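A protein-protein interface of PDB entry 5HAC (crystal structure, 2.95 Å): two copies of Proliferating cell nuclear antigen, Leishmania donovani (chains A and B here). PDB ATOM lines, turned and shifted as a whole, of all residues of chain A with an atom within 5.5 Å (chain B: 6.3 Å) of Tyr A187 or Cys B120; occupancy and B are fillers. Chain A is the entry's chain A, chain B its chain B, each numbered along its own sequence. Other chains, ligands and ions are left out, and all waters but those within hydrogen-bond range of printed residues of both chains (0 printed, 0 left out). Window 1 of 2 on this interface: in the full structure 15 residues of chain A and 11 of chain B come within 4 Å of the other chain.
No position is printed for both chains.
Glu B121 touches Gln A185 (O to O, 3.9 Å). O of Gln A185 touches CA of Tyr B122, at 3.3 Å. O of Glu B121 touches CA of Gly A186 (3.7 Å). Gly A186 touches Tyr B122 (CA to CD1, 3.7 Å). Tyr A187 touches Lys B119. Tyr A187 touches Cys B120. Lys B119 touches Thr A188 (O to CA, 3.7 Å). CA of Arg B118 touches O of Phe A189, at 3.5 Å.
The backbone carbonyl oxygen of Tyr A187 lies within hydrogen-bond range of the backbone NH of Glu B121, 3.0 Å away. The side-chain hydroxyl (OG1) of Thr A188 lies within hydrogen-bond range of the side-chain sulfur (SG) of Cys B120 (3.5 Å). The backbone NH of Phe A189 lies within hydrogen-bond range of the backbone carbonyl oxygen of Lys B119, at 2.8 Å.
Hydrophobic or aromatic side chains of chain B within 4 Å of the printed part of chain A: Tyr B122. Among the printed residues, no Asp or Glu carboxylate lies within 4 Å of a Lys or Arg side-chain nitrogen of the other chain.
Of chain A, only Tyr A187 (3.4 Å) and Thr A188 (3.5 Å) come within 4 Å of Cys B120. Of the printed residues of chain A, Lys B119 touches Tyr A187 (3.2 Å), Thr A188 (3.7 Å) and Phe A189 (2.8 Å). Of the printed residues of chain B, Gln A185 touches Glu B121 (3.9 Å) and Tyr B122 (3.3 Å). Of the printed residues of chain B, Phe A189 touches Arg B118 and Lys B119. Of the printed residues of chain B, Thr A188 touches Lys B119 and Cys B120. Phe A177 touches none of the printed residues of chain B. The nearest residue of chain B that does not touch Tyr A187 is Tyr B122 (4.1 Å). The nearest printed residue of chain B that does not touch Phe A189 is Cys B120 (4.9 Å).
O of Phe A177 lies within hydrogen-bond range of N of Thr A188 (2.8 Å). The backbone NH (N) of Ser A179 is in hydrogen-bond range of the backbone carbonyl oxygen (O) of Gly A186. The guanidinium group (NH2) of Arg B118 lies within salt-bridge range of the side-chain carboxylate (OD2) of Asp B94 (2.9 Å). O of Tyr B122 sits at hydrogen-bond distance from N of Leu B109, at 2.8 Å. O of Ser B111 sits at hydrogen-bond distance from N of Cys B120 (2.8 Å). SG of Cys B120 sits close to OH of Tyr B122, 3.4 Å away.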
ATOM      1  N   MET A 159      30.535 -25.019  25.922  1.00  0.00           N
ATOM      2  CA  MET A 159      30.809 -26.006  24.867  1.00  0.00           C
ATOM      3  C   MET A 159      31.573 -27.251  25.335  1.00  0.00           C
ATOM      4  O   MET A 159      31.449 -28.312  24.729  1.00  0.00           O
ATOM      5  CB  MET A 159      31.596 -25.365  23.717  1.00  0.00           C
ATOM      6  CG  MET A 159      30.847 -24.313  22.922  1.00  0.00           C
ATOM      7  SD  MET A 159      29.431 -24.937  22.014  1.00  0.00           S
ATOM      8  CE  MET A 159      28.110 -24.545  23.180  1.00  0.00           C
ATOM      9  N   LYS A 176      28.625 -18.541  15.210  1.00  0.00           N
ATOM     10  CA  LYS A 176      28.059 -19.739  15.806  1.00  0.00           C
ATOM     11  C   LYS A 176      29.175 -20.664  16.327  1.00  0.00           C
ATOM     12  O   LYS A 176      29.954 -21.218  15.546  1.00  0.00           O
ATOM     13  CB  LYS A 176      27.187 -20.478  14.789  1.00  0.00           C
ATOM     14  CG  LYS A 176      26.863 -21.925  15.153  1.00  0.00           C
ATOM     15  CD  LYS A 176      25.423 -22.325  14.848  1.00  0.00           C
ATOM     16  CE  LYS A 176      25.295 -23.236  13.651  1.00  0.00           C
ATOM     17  NZ  LYS A 176      23.943 -23.856  13.668  1.00  0.00           N
ATOM     18  N   PHE A 177      29.193 -20.857  17.644  1.00  0.00           N
ATOM     19  CA  PHE A 177      30.036 -21.860  18.299  1.00  0.00           C
ATOM     20  C   PHE A 177      29.261 -23.167  18.517  1.00  0.00           C
ATOM     21  O   PHE A 177      28.157 -23.134  19.064  1.00  0.00           O
ATOM     22  CB  PHE A 177      30.459 -21.347  19.642  1.00  0.00           C
ATOM     23  CG  PHE A 177      31.130 -20.017  19.595  1.00  0.00           C
ATOM     24  CD1 PHE A 177      30.397 -18.845  19.651  1.00  0.00           C
ATOM     25  CD2 PHE A 177      32.509 -19.937  19.548  1.00  0.00           C
ATOM     26  CE1 PHE A 177      31.027 -17.620  19.665  1.00  0.00           C
ATOM     27  CE2 PHE A 177      33.158 -18.710  19.546  1.00  0.00           C
ATOM     28  CZ  PHE A 177      32.417 -17.550  19.610  1.00  0.00           C
ATOM     29  N   SER A 178      29.854 -24.299  18.132  1.00  0.00           N
ATOM     30  CA  SER A 178      29.151 -25.600  18.069  1.00  0.00           C
ATOM     31  C   SER A 178      30.006 -26.706  18.676  1.00  0.00           C
ATOM     32  O   SER A 178      31.241 -26.700  18.542  1.00  0.00           O
ATOM     33  CB  SER A 178      28.833 -25.988  16.620  1.00  0.00           C
ATOM     34  OG  SER A 178      28.761 -24.852  15.770  1.00  0.00           O
ATOM     35  N   SER A 179      29.358 -27.692  19.292  1.00  0.00           N
ATOM     36  CA  SER A 179      30.098 -28.831  19.838  1.00  0.00           C
ATOM     37  C   SER A 179      29.265 -30.093  19.882  1.00  0.00           C
ATOM     38  O   SER A 179      28.035 -30.028  19.900  1.00  0.00           O
ATOM     39  CB  SER A 179      30.645 -28.473  21.221  1.00  0.00           C
ATOM     40  OG  SER A 179      31.783 -29.261  21.523  1.00  0.00           O
ATOM     41  N   GLN A 185      24.519 -32.402  21.657  1.00  0.00           N
ATOM     42  CA  GLN A 185      25.015 -31.372  20.754  1.00  0.00           C
ATOM     43  C   GLN A 185      24.542 -30.026  21.191  1.00  0.00           C
ATOM     44  O   GLN A 185      23.367 -29.845  21.474  1.00  0.00           O
ATOM     45  CB  GLN A 185      24.473 -31.572  19.373  1.00  0.00           C
ATOM     46  CG  GLN A 185      24.603 -32.969  18.840  1.00  0.00           C
ATOM     47  CD  GLN A 185      24.207 -33.022  17.396  1.00  0.00           C
ATOM     48  OE1 GLN A 185      23.682 -32.045  16.848  1.00  0.00           O
ATOM     49  NE2 GLN A 185      24.468 -34.146  16.760  1.00  0.00           N
ATOM     50  N   GLY A 186      25.456 -29.074  21.214  1.00  0.00           N
ATOM     51  CA  GLY A 186      25.133 -27.721  21.617  1.00  0.00           C
ATOM     52  C   GLY A 186      25.590 -26.735  20.583  1.00  0.00           C
ATOM     53  O   GLY A 186      26.491 -27.008  19.789  1.00  0.00           O
ATOM     54  N   TYR A 187      24.912 -25.600  20.554  1.00  0.00           N
ATOM     55  CA  TYR A 187      25.467 -24.440  19.896  1.00  0.00           C
ATOM     56  C   TYR A 187      25.037 -23.183  20.598  1.00  0.00           C
ATOM     57  O   TYR A 187      24.024 -23.142  21.290  1.00  0.00           O
ATOM     58  CB  TYR A 187      25.161 -24.408  18.382  1.00  0.00           C
ATOM     59  CG  TYR A 187      23.775 -23.939  17.940  1.00  0.00           C
ATOM     60  CD1 TYR A 187      23.354 -22.624  18.119  1.00  0.00           C
ATOM     61  CD2 TYR A 187      22.910 -24.809  17.275  1.00  0.00           C
ATOM     62  CE1 TYR A 187      22.104 -22.202  17.693  1.00  0.00           C
ATOM     63  CE2 TYR A 187      21.654 -24.397  16.847  1.00  0.00           C
ATOM     64  CZ  TYR A 187      21.250 -23.097  17.061  1.00  0.00           C
ATOM     65  OH  TYR A 187      19.995 -22.700  16.646  1.00  0.00           O
ATOM     66  N   THR A 188      25.864 -22.169  20.450  1.00  0.00           N
ATOM     67  CA  THR A 188      25.544 -20.828  20.897  1.00  0.00           C
ATOM     68  C   THR A 188      25.746 -19.952  19.676  1.00  0.00           C
ATOM     69  O   THR A 188      26.779 -20.031  19.021  1.00  0.00           O
ATOM     70  CB  THR A 188      26.453 -20.405  22.065  1.00  0.00           C
ATOM     71  OG1 THR A 188      26.215 -21.279  23.181  1.00  0.00           O
ATOM     72  CG2 THR A 188      26.176 -18.983  22.490  1.00  0.00           C
ATOM     73  N   PHE A 189      24.729 -19.166  19.346  1.00  0.00           N
ATOM     74  CA  PHE A 189      24.771 -18.256  18.209  1.00  0.00           C
ATOM     75  C   PHE A 189      24.737 -16.847  18.786  1.00  0.00           C
ATOM     76  O   PHE A 189      23.863 -16.539  19.598  1.00  0.00           O
ATOM     77  CB  PHE A 189      23.551 -18.479  17.305  1.00  0.00           C
ATOM     78  CG  PHE A 189      23.621 -17.771  15.966  1.00  0.00           C
ATOM     79  CD1 PHE A 189      23.505 -16.372  15.883  1.00  0.00           C
ATOM     80  CD2 PHE A 189      23.751 -18.505  14.787  1.00  0.00           C
ATOM     81  CE1 PHE A 189      23.561 -15.726  14.670  1.00  0.00           C
ATOM     82  CE2 PHE A 189      23.800 -17.867  13.566  1.00  0.00           C
ATOM     83  CZ  PHE A 189      23.709 -16.484  13.508  1.00  0.00           C
ATOM     84  N   VAL B  90      22.801 -22.914  31.249  1.00  0.00           N
ATOM     85  CA  VAL B  90      21.797 -22.023  30.694  1.00  0.00           C
ATOM     86  C   VAL B  90      21.564 -20.915  31.684  1.00  0.00           C
ATOM     87  O   VAL B  90      21.278 -21.192  32.840  1.00  0.00           O
ATOM     88  CB  VAL B  90      20.470 -22.750  30.457  1.00  0.00           C
ATOM     89  CG1 VAL B  90      19.395 -21.779  30.032  1.00  0.00           C
ATOM     90  CG2 VAL B  90      20.665 -23.785  29.386  1.00  0.00           C
ATOM     91  N   ASP B  94      17.357 -16.287  30.999  1.00  0.00           N
ATOM     92  CA  ASP B  94      16.966 -16.572  29.639  1.00  0.00           C
ATOM     93  C   ASP B  94      15.642 -17.377  29.603  1.00  0.00           C
ATOM     94  O   ASP B  94      15.273 -18.067  30.560  1.00  0.00           O
ATOM     95  CB  ASP B  94      18.105 -17.295  28.900  1.00  0.00           C
ATOM     96  CG  ASP B  94      19.287 -16.367  28.582  1.00  0.00           C
ATOM     97  OD1 ASP B  94      19.242 -15.167  28.968  1.00  0.00           O
ATOM     98  OD2 ASP B  94      20.264 -16.862  27.945  1.00  0.00           O
ATOM     99  N   LEU B 109      16.274 -28.186  23.331  1.00  0.00           N
ATOM    100  CA  LEU B 109      16.142 -27.078  24.255  1.00  0.00           C
ATOM    101  C   LEU B 109      16.672 -25.839  23.604  1.00  0.00           C
ATOM    102  O   LEU B 109      17.790 -25.835  23.109  1.00  0.00           O
ATOM    103  CB  LEU B 109      16.945 -27.364  25.534  1.00  0.00           C
ATOM    104  CG  LEU B 109      16.352 -28.512  26.356  1.00  0.00           C
ATOM    105  CD1 LEU B 109      17.304 -29.000  27.418  1.00  0.00           C
ATOM    106  CD2 LEU B 109      15.058 -28.076  27.014  1.00  0.00           C
ATOM    107  N   THR B 110      15.890 -24.770  23.659  1.00  0.00           N
ATOM    108  CA  THR B 110      16.264 -23.536  22.993  1.00  0.00           C
ATOM    109  C   THR B 110      16.124 -22.380  23.974  1.00  0.00           C
ATOM    110  O   THR B 110      15.080 -22.170  24.588  1.00  0.00           O
ATOM    111  CB  THR B 110      15.436 -23.305  21.715  1.00  0.00           C
ATOM    112  OG1 THR B 110      15.377 -24.515  20.950  1.00  0.00           O
ATOM    113  CG2 THR B 110      16.066 -22.240  20.873  1.00  0.00           C
ATOM    114  N   SER B 111      17.214 -21.655  24.130  1.00  0.00           N
ATOM    115  CA  SER B 111      17.314 -20.586  25.092  1.00  0.00           C
ATOM    116  C   SER B 111      17.563 -19.309  24.342  1.00  0.00           C
ATOM    117  O   SER B 111      18.285 -19.286  23.334  1.00  0.00           O
ATOM    118  CB  SER B 111      18.468 -20.844  26.077  1.00  0.00           C
ATOM    119  OG  SER B 111      19.319 -19.710  26.220  1.00  0.00           O
ATOM    120  N   GLU B 112      17.021 -18.233  24.883  1.00  0.00           N
ATOM    121  CA  GLU B 112      17.214 -16.937  24.309  1.00  0.00           C
ATOM    122  C   GLU B 112      17.174 -15.873  25.402  1.00  0.00           C
ATOM    123  O   GLU B 112      16.375 -15.939  26.332  1.00  0.00           O
ATOM    124  CB  GLU B 112      16.145 -16.709  23.232  1.00  0.00           C
ATOM    125  CG  GLU B 112      16.478 -15.614  22.224  1.00  0.00           C
ATOM    126  CD  GLU B 112      16.107 -15.958  20.781  1.00  0.00           C
ATOM    127  OE1 GLU B 112      16.724 -15.359  19.873  1.00  0.00           O
ATOM    128  OE2 GLU B 112      15.233 -16.824  20.542  1.00  0.00           O
ATOM    129  N   ARG B 118      21.468 -13.236  21.724  1.00  0.00           N
ATOM    130  CA  ARG B 118      22.081 -14.553  21.894  1.00  0.00           C
ATOM    131  C   ARG B 118      20.994 -15.602  21.793  1.00  0.00           C
ATOM    132  O   ARG B 118      19.911 -15.434  22.342  1.00  0.00           O
ATOM    133  CB  ARG B 118      22.793 -14.670  23.257  1.00  0.00           C
ATOM    134  CG  ARG B 118      23.083 -16.110  23.727  1.00  0.00           C
ATOM    135  CD  ARG B 118      24.174 -16.219  24.794  1.00  0.00           C
ATOM    136  NE  ARG B 118      23.653 -16.524  26.131  1.00  0.00           N
ATOM    137  CZ  ARG B 118      23.546 -15.677  27.157  1.00  0.00           C
ATOM    138  NH1 ARG B 118      23.917 -14.412  27.063  1.00  0.00           N
ATOM    139  NH2 ARG B 118      23.062 -16.110  28.321  1.00  0.00           N
ATOM    140  N   LYS B 119      21.303 -16.701  21.124  1.00  0.00           N
ATOM    141  CA  LYS B 119      20.398 -17.835  21.068  1.00  0.00           C
ATOM    142  C   LYS B 119      21.189 -19.130  21.197  1.00  0.00           C
ATOM    143  O   LYS B 119      22.168 -19.339  20.469  1.00  0.00           O
ATOM    144  CB  LYS B 119      19.586 -17.822  19.761  1.00  0.00           C
ATOM    145  CG  LYS B 119      18.922 -19.151  19.424  1.00  0.00           C
ATOM    146  CD  LYS B 119      17.948 -19.074  18.261  1.00  0.00           C
ATOM    147  CE  LYS B 119      18.034 -20.345  17.428  1.00  0.00           C
ATOM    148  NZ  LYS B 119      16.716 -20.749  16.868  1.00  0.00           N
ATOM    149  N   CYS B 120      20.724 -20.000  22.094  1.00  0.00           N
ATOM    150  CA  CYS B 120      21.384 -21.258  22.367  1.00  0.00           C
ATOM    151  C   CYS B 120      20.458 -22.381  22.037  1.00  0.00           C
ATOM    152  O   CYS B 120      19.256 -22.262  22.248  1.00  0.00           O
ATOM    153  CB  CYS B 120      21.749 -21.335  23.820  1.00  0.00           C
ATOM    154  SG  CYS B 120      23.040 -20.152  24.196  1.00  0.00           S
ATOM    155  N   GLU B 121      21.008 -23.464  21.482  1.00  0.00           N
ATOM    156  CA  GLU B 121      20.203 -24.641  21.194  1.00  0.00           C
ATOM    157  C   GLU B 121      20.929 -25.954  21.398  1.00  0.00           C
ATOM    158  O   GLU B 121      21.892 -26.298  20.705  1.00  0.00           O
ATOM    159  CB  GLU B 121      19.617 -24.595  19.791  1.00  0.00           C
ATOM    160  CG  GLU B 121      18.437 -25.529  19.629  1.00  0.00           C
ATOM    161  CD  GLU B 121      17.975 -25.588  18.206  1.00  0.00           C
ATOM    162  OE1 GLU B 121      17.065 -24.782  17.857  1.00  0.00           O
ATOM    163  OE2 GLU B 121      18.557 -26.410  17.443  1.00  0.00           O
ATOM    164  N   TYR B 122      20.397 -26.700  22.347  1.00  0.00           N
ATOM    165  CA  TYR B 122      20.959 -27.947  22.778  1.00  0.00           C
ATOM    166  C   TYR B 122      20.008 -29.068  22.384  1.00  0.00           C
ATOM    167  O   TYR B 122      18.793 -28.911  22.480  1.00  0.00           O
ATOM    168  CB  TYR B 122      21.175 -27.888  24.296  1.00  0.00           C
ATOM    169  CG  TYR B 122      21.857 -26.612  24.751  1.00  0.00           C
ATOM    170  CD1 TYR B 122      23.200 -26.378  24.472  1.00  0.00           C
ATOM    171  CD2 TYR B 122      21.160 -25.621  25.443  1.00  0.00           C
ATOM    172  CE1 TYR B 122      23.832 -25.193  24.873  1.00  0.00           C
ATOM    173  CE2 TYR B 122      21.791 -24.429  25.866  1.00  0.00           C
ATOM    174  CZ  TYR B 122      23.127 -24.210  25.590  1.00  0.00           C
ATOM    175  OH  TYR B 122      23.760 -23.022  25.957  1.00  0.00           O
